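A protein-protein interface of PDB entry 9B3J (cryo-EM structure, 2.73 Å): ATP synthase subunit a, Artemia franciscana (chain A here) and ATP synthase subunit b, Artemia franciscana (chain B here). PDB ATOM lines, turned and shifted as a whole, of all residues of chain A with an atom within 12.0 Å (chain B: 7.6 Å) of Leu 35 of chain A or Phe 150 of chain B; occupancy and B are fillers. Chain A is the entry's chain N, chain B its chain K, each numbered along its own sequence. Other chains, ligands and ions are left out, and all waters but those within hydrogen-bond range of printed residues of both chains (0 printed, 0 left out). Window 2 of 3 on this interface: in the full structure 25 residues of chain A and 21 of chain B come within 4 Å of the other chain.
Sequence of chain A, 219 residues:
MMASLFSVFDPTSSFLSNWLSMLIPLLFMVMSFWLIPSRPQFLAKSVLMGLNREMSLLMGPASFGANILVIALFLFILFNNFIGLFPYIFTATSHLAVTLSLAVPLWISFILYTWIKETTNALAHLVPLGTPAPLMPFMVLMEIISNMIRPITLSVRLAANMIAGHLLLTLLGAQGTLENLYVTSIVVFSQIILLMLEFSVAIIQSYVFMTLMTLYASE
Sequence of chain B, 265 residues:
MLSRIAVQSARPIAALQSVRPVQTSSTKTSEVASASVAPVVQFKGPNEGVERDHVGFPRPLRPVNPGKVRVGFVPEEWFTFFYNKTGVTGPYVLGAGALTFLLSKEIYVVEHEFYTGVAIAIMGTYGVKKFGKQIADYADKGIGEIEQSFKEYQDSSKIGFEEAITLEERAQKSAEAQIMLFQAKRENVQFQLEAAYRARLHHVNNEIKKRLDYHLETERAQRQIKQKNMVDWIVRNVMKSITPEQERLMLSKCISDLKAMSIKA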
ATOM      1  N   MET A  31     -17.985  17.146 -22.930  1.00  0.00           N
ATOM      2  CA  MET A  31     -19.281  17.190 -22.280  1.00  0.00           C
ATOM      3  C   MET A  31     -20.266  16.349 -23.074  1.00  0.00           C
ATOM      4  O   MET A  31     -20.302  16.419 -24.305  1.00  0.00           O
ATOM      5  CB  MET A  31     -19.786  18.626 -22.160  1.00  0.00           C
ATOM      6  CG  MET A  31     -19.273  19.363 -20.940  1.00  0.00           C
ATOM      7  SD  MET A  31     -19.942  21.032 -20.869  1.00  0.00           S
ATOM      8  CE  MET A  31     -19.387  21.558 -19.257  1.00  0.00           C
ATOM      9  N   SER A  32     -21.063  15.560 -22.361  1.00  0.00           N
ATOM     10  CA  SER A  32     -21.948  14.571 -22.960  1.00  0.00           C
ATOM     11  C   SER A  32     -23.392  15.033 -22.838  1.00  0.00           C
ATOM     12  O   SER A  32     -23.883  15.256 -21.732  1.00  0.00           O
ATOM     13  CB  SER A  32     -21.758  13.213 -22.293  1.00  0.00           C
ATOM     14  OG  SER A  32     -21.797  13.335 -20.886  1.00  0.00           O
ATOM     15  N   PHE A  33     -24.063  15.171 -23.974  1.00  0.00           N
ATOM     16  CA  PHE A  33     -25.467  15.547 -24.020  1.00  0.00           C
ATOM     17  C   PHE A  33     -26.333  14.483 -24.668  1.00  0.00           C
ATOM     18  O   PHE A  33     -27.320  14.048 -24.069  1.00  0.00           O
ATOM     19  CB  PHE A  33     -25.621  16.874 -24.768  1.00  0.00           C
ATOM     20  CG  PHE A  33     -27.027  17.361 -24.868  1.00  0.00           C
ATOM     21  CD1 PHE A  33     -27.590  18.073 -23.849  1.00  0.00           C
ATOM     22  CD2 PHE A  33     -27.764  17.154 -26.004  1.00  0.00           C
ATOM     23  CE1 PHE A  33     -28.872  18.540 -23.948  1.00  0.00           C
ATOM     24  CE2 PHE A  33     -29.047  17.617 -26.101  1.00  0.00           C
ATOM     25  CZ  PHE A  33     -29.598  18.311 -25.073  1.00  0.00           C
ATOM     26  N   TRP A  34     -25.999  14.046 -25.877  1.00  0.00           N
ATOM     27  CA  TRP A  34     -26.854  13.095 -26.565  1.00  0.00           C
ATOM     28  C   TRP A  34     -26.531  11.672 -26.135  1.00  0.00           C
ATOM     29  O   TRP A  34     -25.465  11.388 -25.585  1.00  0.00           O
ATOM     30  CB  TRP A  34     -26.703  13.216 -28.074  1.00  0.00           C
ATOM     31  CG  TRP A  34     -27.096  14.531 -28.630  1.00  0.00           C
ATOM     32  CD1 TRP A  34     -26.264  15.518 -29.036  1.00  0.00           C
ATOM     33  CD2 TRP A  34     -28.424  15.005 -28.857  1.00  0.00           C
ATOM     34  NE1 TRP A  34     -26.987  16.582 -29.502  1.00  0.00           N
ATOM     35  CE2 TRP A  34     -28.318  16.289 -29.402  1.00  0.00           C
ATOM     36  CE3 TRP A  34     -29.690  14.467 -28.655  1.00  0.00           C
ATOM     37  CZ2 TRP A  34     -29.424  17.042 -29.745  1.00  0.00           C
ATOM     38  CZ3 TRP A  34     -30.785  15.218 -28.998  1.00  0.00           C
ATOM     39  CH2 TRP A  34     -30.647  16.490 -29.534  1.00  0.00           C
ATOM     40  N   LEU A  35     -27.476  10.769 -26.397  1.00  0.00           N
ATOM     41  CA  LEU A  35     -27.314   9.386 -25.966  1.00  0.00           C
ATOM     42  C   LEU A  35     -26.239   8.680 -26.774  1.00  0.00           C
ATOM     43  O   LEU A  35     -25.375   7.999 -26.215  1.00  0.00           O
ATOM     44  CB  LEU A  35     -28.641   8.644 -26.075  1.00  0.00           C
ATOM     45  CG  LEU A  35     -28.592   7.158 -25.750  1.00  0.00           C
ATOM     46  CD1 LEU A  35     -28.175   6.938 -24.316  1.00  0.00           C
ATOM     47  CD2 LEU A  35     -29.946   6.557 -26.005  1.00  0.00           C
ATOM     48  N   ILE A  36     -26.281   8.824 -28.093  1.00  0.00           N
ATOM     49  CA  ILE A  36     -25.229   8.308 -28.960  1.00  0.00           C
ATOM     50  C   ILE A  36     -24.134   9.361 -29.010  1.00  0.00           C
ATOM     51  O   ILE A  36     -24.401  10.508 -29.384  1.00  0.00           O
ATOM     52  CB  ILE A  36     -25.763   7.976 -30.358  1.00  0.00           C
ATOM     53  CG1 ILE A  36     -26.895   8.932 -30.726  1.00  0.00           C
ATOM     54  CG2 ILE A  36     -26.242   6.542 -30.410  1.00  0.00           C
ATOM     55  CD1 ILE A  36     -27.371   8.776 -32.138  1.00  0.00           C
ATOM     56  N   PRO A  37     -22.907   9.029 -28.636  1.00  0.00           N
ATOM     57  CA  PRO A  37     -21.889  10.063 -28.435  1.00  0.00           C
ATOM     58  C   PRO A  37     -21.412  10.654 -29.752  1.00  0.00           C
ATOM     59  O   PRO A  37     -21.675  10.137 -30.835  1.00  0.00           O
ATOM     60  CB  PRO A  37     -20.764   9.318 -27.714  1.00  0.00           C
ATOM     61  CG  PRO A  37     -20.983   7.895 -28.005  1.00  0.00           C
ATOM     62  CD  PRO A  37     -22.431   7.689 -28.272  1.00  0.00           C
ATOM     63  N   SER A  38     -20.724  11.784 -29.643  1.00  0.00           N
ATOM     64  CA  SER A  38     -20.086  12.378 -30.803  1.00  0.00           C
ATOM     65  C   SER A  38     -18.735  11.719 -31.034  1.00  0.00           C
ATOM     66  O   SER A  38     -18.341  10.790 -30.326  1.00  0.00           O
ATOM     67  CB  SER A  38     -19.935  13.881 -30.616  1.00  0.00           C
ATOM     68  OG  SER A  38     -19.177  14.158 -29.456  1.00  0.00           O
ATOM     69  N   ARG A  39     -18.022  12.188 -32.052  1.00  0.00           N
ATOM     70  CA  ARG A  39     -16.671  11.684 -32.294  1.00  0.00           C
ATOM     71  C   ARG A  39     -15.691  11.970 -31.157  1.00  0.00           C
ATOM     72  O   ARG A  39     -14.991  11.028 -30.743  1.00  0.00           O
ATOM     73  CB  ARG A  39     -16.152  12.220 -33.629  1.00  0.00           C
ATOM     74  CG  ARG A  39     -16.957  11.779 -34.822  1.00  0.00           C
ATOM     75  CD  ARG A  39     -16.447  12.436 -36.083  1.00  0.00           C
ATOM     76  NE  ARG A  39     -17.076  11.890 -37.277  1.00  0.00           N
ATOM     77  CZ  ARG A  39     -16.879  12.356 -38.502  1.00  0.00           C
ATOM     78  NH1 ARG A  39     -16.093  13.393 -38.727  1.00  0.00           N
ATOM     79  NH2 ARG A  39     -17.488  11.766 -39.525  1.00  0.00           N
ATOM     80  N   PRO A  40     -15.569  13.195 -30.607  1.00  0.00           N
ATOM     81  CA  PRO A  40     -14.560  13.380 -29.556  1.00  0.00           C
ATOM     82  C   PRO A  40     -14.923  12.708 -28.252  1.00  0.00           C
ATOM     83  O   PRO A  40     -14.025  12.218 -27.560  1.00  0.00           O
ATOM     84  CB  PRO A  40     -14.486  14.902 -29.402  1.00  0.00           C
ATOM     85  CG  PRO A  40     -15.809  15.362 -29.765  1.00  0.00           C
ATOM     86  CD  PRO A  40     -16.233  14.486 -30.895  1.00  0.00           C
ATOM     87  N   GLN A  41     -16.209  12.664 -27.900  1.00  0.00           N
ATOM     88  CA  GLN A  41     -16.621  11.978 -26.684  1.00  0.00           C
ATOM     89  C   GLN A  41     -16.349  10.488 -26.780  1.00  0.00           C
ATOM     90  O   GLN A  41     -15.859   9.878 -25.825  1.00  0.00           O
ATOM     91  CB  GLN A  41     -18.098  12.227 -26.418  1.00  0.00           C
ATOM     92  CG  GLN A  41     -18.616  11.501 -25.207  1.00  0.00           C
ATOM     93  CD  GLN A  41     -20.112  11.585 -25.087  1.00  0.00           C
ATOM     94  OE1 GLN A  41     -20.757  12.419 -25.722  1.00  0.00           O
ATOM     95  NE2 GLN A  41     -20.681  10.703 -24.281  1.00  0.00           N
ATOM     96  N   PHE A  42     -16.646   9.888 -27.932  1.00  0.00           N
ATOM     97  CA  PHE A  42     -16.373   8.469 -28.108  1.00  0.00           C
ATOM     98  C   PHE A  42     -14.881   8.189 -28.096  1.00  0.00           C
ATOM     99  O   PHE A  42     -14.444   7.183 -27.531  1.00  0.00           O
ATOM    100  CB  PHE A  42     -16.993   7.954 -29.402  1.00  0.00           C
ATOM    101  CG  PHE A  42     -16.652   6.528 -29.697  1.00  0.00           C
ATOM    102  CD1 PHE A  42     -17.248   5.508 -28.985  1.00  0.00           C
ATOM    103  CD2 PHE A  42     -15.723   6.203 -30.668  1.00  0.00           C
ATOM    104  CE1 PHE A  42     -16.931   4.193 -29.240  1.00  0.00           C
ATOM    105  CE2 PHE A  42     -15.401   4.891 -30.925  1.00  0.00           C
ATOM    106  CZ  PHE A  42     -16.008   3.885 -30.212  1.00  0.00           C
ATOM    107  N   LEU A  43     -14.084   9.062 -28.714  1.00  0.00           N
ATOM    108  CA  LEU A  43     -12.639   8.851 -28.721  1.00  0.00           C
ATOM    109  C   LEU A  43     -12.044   8.997 -27.326  1.00  0.00           C
ATOM    110  O   LEU A  43     -11.178   8.204 -26.925  1.00  0.00           O
ATOM    111  CB  LEU A  43     -11.982   9.825 -29.689  1.00  0.00           C
ATOM    112  CG  LEU A  43     -12.152   9.487 -31.162  1.00  0.00           C
ATOM    113  CD1 LEU A  43     -11.879  10.719 -31.987  1.00  0.00           C
ATOM    114  CD2 LEU A  43     -11.220   8.362 -31.543  1.00  0.00           C
ATOM    115  N   LYS A  45     -13.689   8.524 -24.468  1.00  0.00           N
ATOM    116  CA  LYS A  45     -14.140   7.396 -23.667  1.00  0.00           C
ATOM    117  C   LYS A  45     -13.426   6.112 -24.056  1.00  0.00           C
ATOM    118  O   LYS A  45     -13.152   5.280 -23.192  1.00  0.00           O
ATOM    119  CB  LYS A  45     -15.648   7.214 -23.797  1.00  0.00           C
ATOM    120  CG  LYS A  45     -16.222   6.379 -22.678  1.00  0.00           C
ATOM    121  CD  LYS A  45     -17.286   5.430 -23.166  1.00  0.00           C
ATOM    122  CE  LYS A  45     -17.623   4.414 -22.089  1.00  0.00           C
ATOM    123  NZ  LYS A  45     -18.672   3.463 -22.544  1.00  0.00           N
ATOM    124  N   ARG B  62     -30.248  17.066 -33.390  1.00  0.00           N
ATOM    125  CA  ARG B  62     -28.821  16.847 -33.555  1.00  0.00           C
ATOM    126  C   ARG B  62     -28.473  16.910 -35.029  1.00  0.00           C
ATOM    127  O   ARG B  62     -28.797  15.972 -35.772  1.00  0.00           O
ATOM    128  CB  ARG B  62     -28.418  15.497 -32.975  1.00  0.00           C
ATOM    129  CG  ARG B  62     -26.933  15.301 -32.904  1.00  0.00           C
ATOM    130  CD  ARG B  62     -26.601  14.045 -32.158  1.00  0.00           C
ATOM    131  NE  ARG B  62     -25.230  14.066 -31.678  1.00  0.00           N
ATOM    132  CZ  ARG B  62     -24.609  13.009 -31.185  1.00  0.00           C
ATOM    133  NH1 ARG B  62     -25.213  11.841 -31.091  1.00  0.00           N
ATOM    134  NH2 ARG B  62     -23.349  13.123 -30.787  1.00  0.00           N
ATOM    135  N   ILE B 143     -19.798   4.771 -33.376  1.00  0.00           N
ATOM    136  CA  ILE B 143     -21.134   5.327 -33.152  1.00  0.00           C
ATOM    137  C   ILE B 143     -22.180   4.512 -33.901  1.00  0.00           C
ATOM    138  O   ILE B 143     -23.293   4.291 -33.402  1.00  0.00           O
ATOM    139  CB  ILE B 143     -21.190   6.811 -33.562  1.00  0.00           C
ATOM    140  CG1 ILE B 143     -20.103   7.623 -32.866  1.00  0.00           C
ATOM    141  CG2 ILE B 143     -22.541   7.413 -33.245  1.00  0.00           C
ATOM    142  CD1 ILE B 143     -20.015   7.399 -31.410  1.00  0.00           C
ATOM    143  N   GLY B 144     -21.842   4.045 -35.104  1.00  0.00           N
ATOM    144  CA  GLY B 144     -22.746   3.165 -35.821  1.00  0.00           C
ATOM    145  C   GLY B 144     -22.952   1.837 -35.119  1.00  0.00           C
ATOM    146  O   GLY B 144     -24.061   1.308 -35.106  1.00  0.00           O
ATOM    147  N   GLU B 145     -21.889   1.286 -34.523  1.00  0.00           N
ATOM    148  CA  GLU B 145     -22.023   0.041 -33.770  1.00  0.00           C
ATOM    149  C   GLU B 145     -22.918   0.219 -32.552  1.00  0.00           C
ATOM    150  O   GLU B 145     -23.722  -0.665 -32.229  1.00  0.00           O
ATOM    151  CB  GLU B 145     -20.651  -0.469 -33.341  1.00  0.00           C
ATOM    152  CG  GLU B 145     -19.845  -1.097 -34.459  1.00  0.00           C
ATOM    153  CD  GLU B 145     -18.498  -1.612 -33.990  1.00  0.00           C
ATOM    154  OE1 GLU B 145     -18.263  -1.645 -32.763  1.00  0.00           O
ATOM    155  OE2 GLU B 145     -17.671  -1.987 -34.848  1.00  0.00           O
ATOM    156  N   ILE B 146     -22.798   1.357 -31.868  1.00  0.00           N
ATOM    157  CA  ILE B 146     -23.648   1.618 -30.707  1.00  0.00           C
ATOM    158  C   ILE B 146     -25.104   1.785 -31.129  1.00  0.00           C
ATOM    159  O   ILE B 146     -26.017   1.204 -30.524  1.00  0.00           O
ATOM    160  CB  ILE B 146     -23.137   2.846 -29.938  1.00  0.00           C
ATOM    161  CG1 ILE B 146     -21.799   2.532 -29.276  1.00  0.00           C
ATOM    162  CG2 ILE B 146     -24.137   3.274 -28.895  1.00  0.00           C
ATOM    163  CD1 ILE B 146     -21.216   3.687 -28.515  1.00  0.00           C
ATOM    164  N   GLU B 147     -25.345   2.574 -32.180  1.00  0.00           N
ATOM    165  CA  GLU B 147     -26.710   2.779 -32.652  1.00  0.00           C
ATOM    166  C   GLU B 147     -27.312   1.493 -33.204  1.00  0.00           C
ATOM    167  O   GLU B 147     -28.513   1.242 -33.033  1.00  0.00           O
ATOM    168  CB  GLU B 147     -26.729   3.883 -33.705  1.00  0.00           C
ATOM    169  CG  GLU B 147     -28.106   4.274 -34.189  1.00  0.00           C
ATOM    170  CD  GLU B 147     -28.066   5.457 -35.136  1.00  0.00           C
ATOM    171  OE1 GLU B 147     -27.251   6.373 -34.911  1.00  0.00           O
ATOM    172  OE2 GLU B 147     -28.844   5.467 -36.113  1.00  0.00           O
ATOM    173  N   GLN B 148     -26.492   0.658 -33.844  1.00  0.00           N
ATOM    174  CA  GLN B 148     -26.951  -0.643 -34.313  1.00  0.00           C
ATOM    175  C   GLN B 148     -27.325  -1.541 -33.148  1.00  0.00           C
ATOM    176  O   GLN B 148     -28.322  -2.265 -33.216  1.00  0.00           O
ATOM    177  CB  GLN B 148     -25.867  -1.296 -35.169  1.00  0.00           C
ATOM    178  CG  GLN B 148     -26.198  -2.685 -35.673  1.00  0.00           C
ATOM    179  CD  GLN B 148     -25.087  -3.257 -36.525  1.00  0.00           C
ATOM    180  OE1 GLN B 148     -24.197  -2.532 -36.969  1.00  0.00           O
ATOM    181  NE2 GLN B 148     -25.126  -4.565 -36.755  1.00  0.00           N
ATOM    182  N   SER B 149     -26.542  -1.502 -32.067  1.00  0.00           N
ATOM    183  CA  SER B 149     -26.860  -2.316 -30.899  1.00  0.00           C
ATOM    184  C   SER B 149     -28.153  -1.858 -30.235  1.00  0.00           C
ATOM    185  O   SER B 149     -28.939  -2.687 -29.758  1.00  0.00           O
ATOM    186  CB  SER B 149     -25.703  -2.276 -29.906  1.00  0.00           C
ATOM    187  OG  SER B 149     -25.543  -0.975 -29.377  1.00  0.00           O
ATOM    188  N   PHE B 150     -28.399  -0.548 -30.208  1.00  0.00           N
ATOM    189  CA  PHE B 150     -29.656  -0.060 -29.640  1.00  0.00           C
ATOM    190  C   PHE B 150     -30.851  -0.436 -30.512  1.00  0.00           C
ATOM    191  O   PHE B 150     -31.925  -0.794 -29.998  1.00  0.00           O
ATOM    192  CB  PHE B 150     -29.596   1.450 -29.444  1.00  0.00           C
ATOM    193  CG  PHE B 150     -29.038   1.866 -28.116  1.00  0.00           C
ATOM    194  CD1 PHE B 150     -27.675   1.863 -27.891  1.00  0.00           C
ATOM    195  CD2 PHE B 150     -29.879   2.264 -27.095  1.00  0.00           C
ATOM    196  CE1 PHE B 150     -27.161   2.247 -26.674  1.00  0.00           C
ATOM    197  CE2 PHE B 150     -29.369   2.649 -25.873  1.00  0.00           C
ATOM    198  CZ  PHE B 150     -28.008   2.641 -25.664  1.00  0.00           C
ATOM    199  N   LYS B 151     -30.686  -0.370 -31.834  1.00  0.00           N
ATOM    200  CA  LYS B 151     -31.767  -0.772 -32.728  1.00  0.00           C
ATOM    201  C   LYS B 151     -32.038  -2.270 -32.635  1.00  0.00           C
ATOM    202  O   LYS B 151     -33.201  -2.704 -32.671  1.00  0.00           O
ATOM    203  CB  LYS B 151     -31.428  -0.368 -34.159  1.00  0.00           C
ATOM    204  CG  LYS B 151     -32.541  -0.609 -35.151  1.00  0.00           C
ATOM    205  CD  LYS B 151     -32.106  -0.215 -36.549  1.00  0.00           C
ATOM    206  CE  LYS B 151     -33.201  -0.482 -37.564  1.00  0.00           C
ATOM    207  NZ  LYS B 151     -32.768  -0.112 -38.938  1.00  0.00           N
ATOM    208  N   GLU B 152     -30.979  -3.076 -32.509  1.00  0.00           N
ATOM    209  CA  GLU B 152     -31.147  -4.514 -32.336  1.00  0.00           C
ATOM    210  C   GLU B 152     -31.841  -4.836 -31.023  1.00  0.00           C
ATOM    211  O   GLU B 152     -32.632  -5.784 -30.951  1.00  0.00           O
ATOM    212  CB  GLU B 152     -29.794  -5.219 -32.400  1.00  0.00           C
ATOM    213  CG  GLU B 152     -29.228  -5.353 -33.795  1.00  0.00           C
ATOM    214  CD  GLU B 152     -27.942  -6.147 -33.817  1.00  0.00           C
ATOM    215  OE1 GLU B 152     -27.538  -6.653 -32.751  1.00  0.00           O
ATOM    216  OE2 GLU B 152     -27.334  -6.264 -34.900  1.00  0.00           O
ATOM    217  N   TYR B 153     -31.552  -4.059 -29.973  1.00  0.00           N
ATOM    218  CA  TYR B 153     -32.255  -4.242 -28.707  1.00  0.00           C
ATOM    219  C   TYR B 153     -33.745  -3.973 -28.852  1.00  0.00           C
ATOM    220  O   TYR B 153     -34.573  -4.725 -28.317  1.00  0.00           O
ATOM    221  CB  TYR B 153     -31.661  -3.331 -27.637  1.00  0.00           C
ATOM    222  CG  TYR B 153     -32.638  -2.983 -26.535  1.00  0.00           C
ATOM    223  CD1 TYR B 153     -32.928  -3.892 -25.530  1.00  0.00           C
ATOM    224  CD2 TYR B 153     -33.265  -1.739 -26.496  1.00  0.00           C
ATOM    225  CE1 TYR B 153     -33.820  -3.579 -24.525  1.00  0.00           C
ATOM    226  CE2 TYR B 153     -34.157  -1.424 -25.499  1.00  0.00           C
ATOM    227  CZ  TYR B 153     -34.429  -2.346 -24.516  1.00  0.00           C
ATOM    228  OH  TYR B 153     -35.317  -2.036 -23.515  1.00  0.00           O
ATOM    229  N   GLN B 154     -34.104  -2.892 -29.552  1.00  0.00           N
ATOM    230  CA  GLN B 154     -35.522  -2.566 -29.719  1.00  0.00           C
ATOM    231  C   GLN B 154     -36.256  -3.627 -30.534  1.00  0.00           C
ATOM    232  O   GLN B 154     -37.385  -4.022 -30.192  1.00  0.00           O
ATOM    233  CB  GLN B 154     -35.669  -1.202 -30.377  1.00  0.00           C
ATOM    234  CG  GLN B 154     -37.106  -0.778 -30.550  1.00  0.00           C
ATOM    235  CD  GLN B 154     -37.235   0.533 -31.283  1.00  0.00           C
ATOM    236  OE1 GLN B 154     -36.240   1.125 -31.701  1.00  0.00           O
ATOM    237  NE2 GLN B 154     -38.466   0.996 -31.447  1.00  0.00           N
ATOM    238  N   ASP B 155     -35.625  -4.110 -31.607  1.00  0.00           N
ATOM    239  CA  ASP B 155     -36.247  -5.156 -32.414  1.00  0.00           C
ATOM    240  C   ASP B 155     -36.391  -6.458 -31.633  1.00  0.00           C
ATOM    241  O   ASP B 155     -37.418  -7.141 -31.741  1.00  0.00           O
ATOM    242  CB  ASP B 155     -35.441  -5.383 -33.687  1.00  0.00           C
ATOM    243  CG  ASP B 155     -35.324  -4.132 -34.522  1.00  0.00           C
ATOM    244  OD1 ASP B 155     -36.220  -3.268 -34.421  1.00  0.00           O
ATOM    245  OD2 ASP B 155     -34.336  -4.010 -35.275  1.00  0.00           O
ATOM    246  N   SER B 156     -35.376  -6.813 -30.840  1.00  0.00           N
ATOM    247  CA  SER B 156     -35.449  -8.041 -30.059  1.00  0.00           C
ATOM    248  C   SER B 156     -36.522  -7.953 -28.983  1.00  0.00           C
ATOM    249  O   SER B 156     -37.185  -8.952 -28.683  1.00  0.00           O
ATOM    250  CB  SER B 156     -34.092  -8.346 -29.433  1.00  0.00           C
ATOM    251  OG  SER B 156     -33.737  -7.344 -28.500  1.00  0.00           O
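NH2 of Arg 62 of chain B lies close to O of Ile 36 of chain A, 3.1 Å away.
The backbone carbonyl oxygen of Pro 37 of chain A lies close to the guanidinium group of Arg 62 of chain B, at 3.4 Å.
The guanidinium group of Arg 62 of chain B lies close to the backbone NH of Ser 38 of chain A.
Among the printed residues, merely in contact across the chains: Trp 34 of chain A with Arg 62 of chain B, Leu 35 of chain A with Phe 150 of chain B, Ile 36 of chain A with Glu 147 of chain B, Pro 37 of chain A with Ile 143 of chain B, Ser 38 of chain A with Ile 143 of chain B and Phe 42 of chain A with Ile 143 of chain B.
Of chain B, only Phe 150 (3.95 Å) comes within 4 Å of Leu 35 of chain A.
Of chain A, only Leu 35 (3.95 Å) comes within 4 Å of Phe 150 of chain B.
No residue of chain A comes within 4 Å of Ile 146 of chain B.
Glu 147 of chain B touches one residue of chain A.
No residue of chain A comes within 4 Å of Ser 149 of chain B.
No residue of chain A comes within 4 Å of Glu 152 of chain B.
No residue of chain A comes within 4 Å of Tyr 153 of chain B.
No residue of chain A comes within 4 Å of Gln 154 of chain B.
Of the printed residues of chain A, Arg 62 of chain B touches Trp 34 (3.2 Å), Ile 36 (2.3 Å), Pro 37 (3.3 Å) and Ser 38 (3.2 Å).
Of the printed residues of chain B, Phe 42 of chain A touches Ile 143.
Printed residues of chain B within 4 Å of Trp 34 of chain A: Arg 62 (3.2 Å).
Printed residues of chain B within 4 Å of Pro 37 of chain A: Arg 62 and Ile 143.
Gly 144 of chain B touches none of the printed residues of chain A.
The nearest residue of chain A that does not touch Phe 150 of chain B is Ile 36 of chain A (5.5 Å).
The nearest printed residue of chain B that does not touch Trp 34 of chain A is Ile 143 of chain B (8.8 Å).
Hydrophobic or aromatic side chains of chain B that line the printed part of chain A: Ile 143 and Phe 150.
Among the printed residues, 9 pairs touch across the chains.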
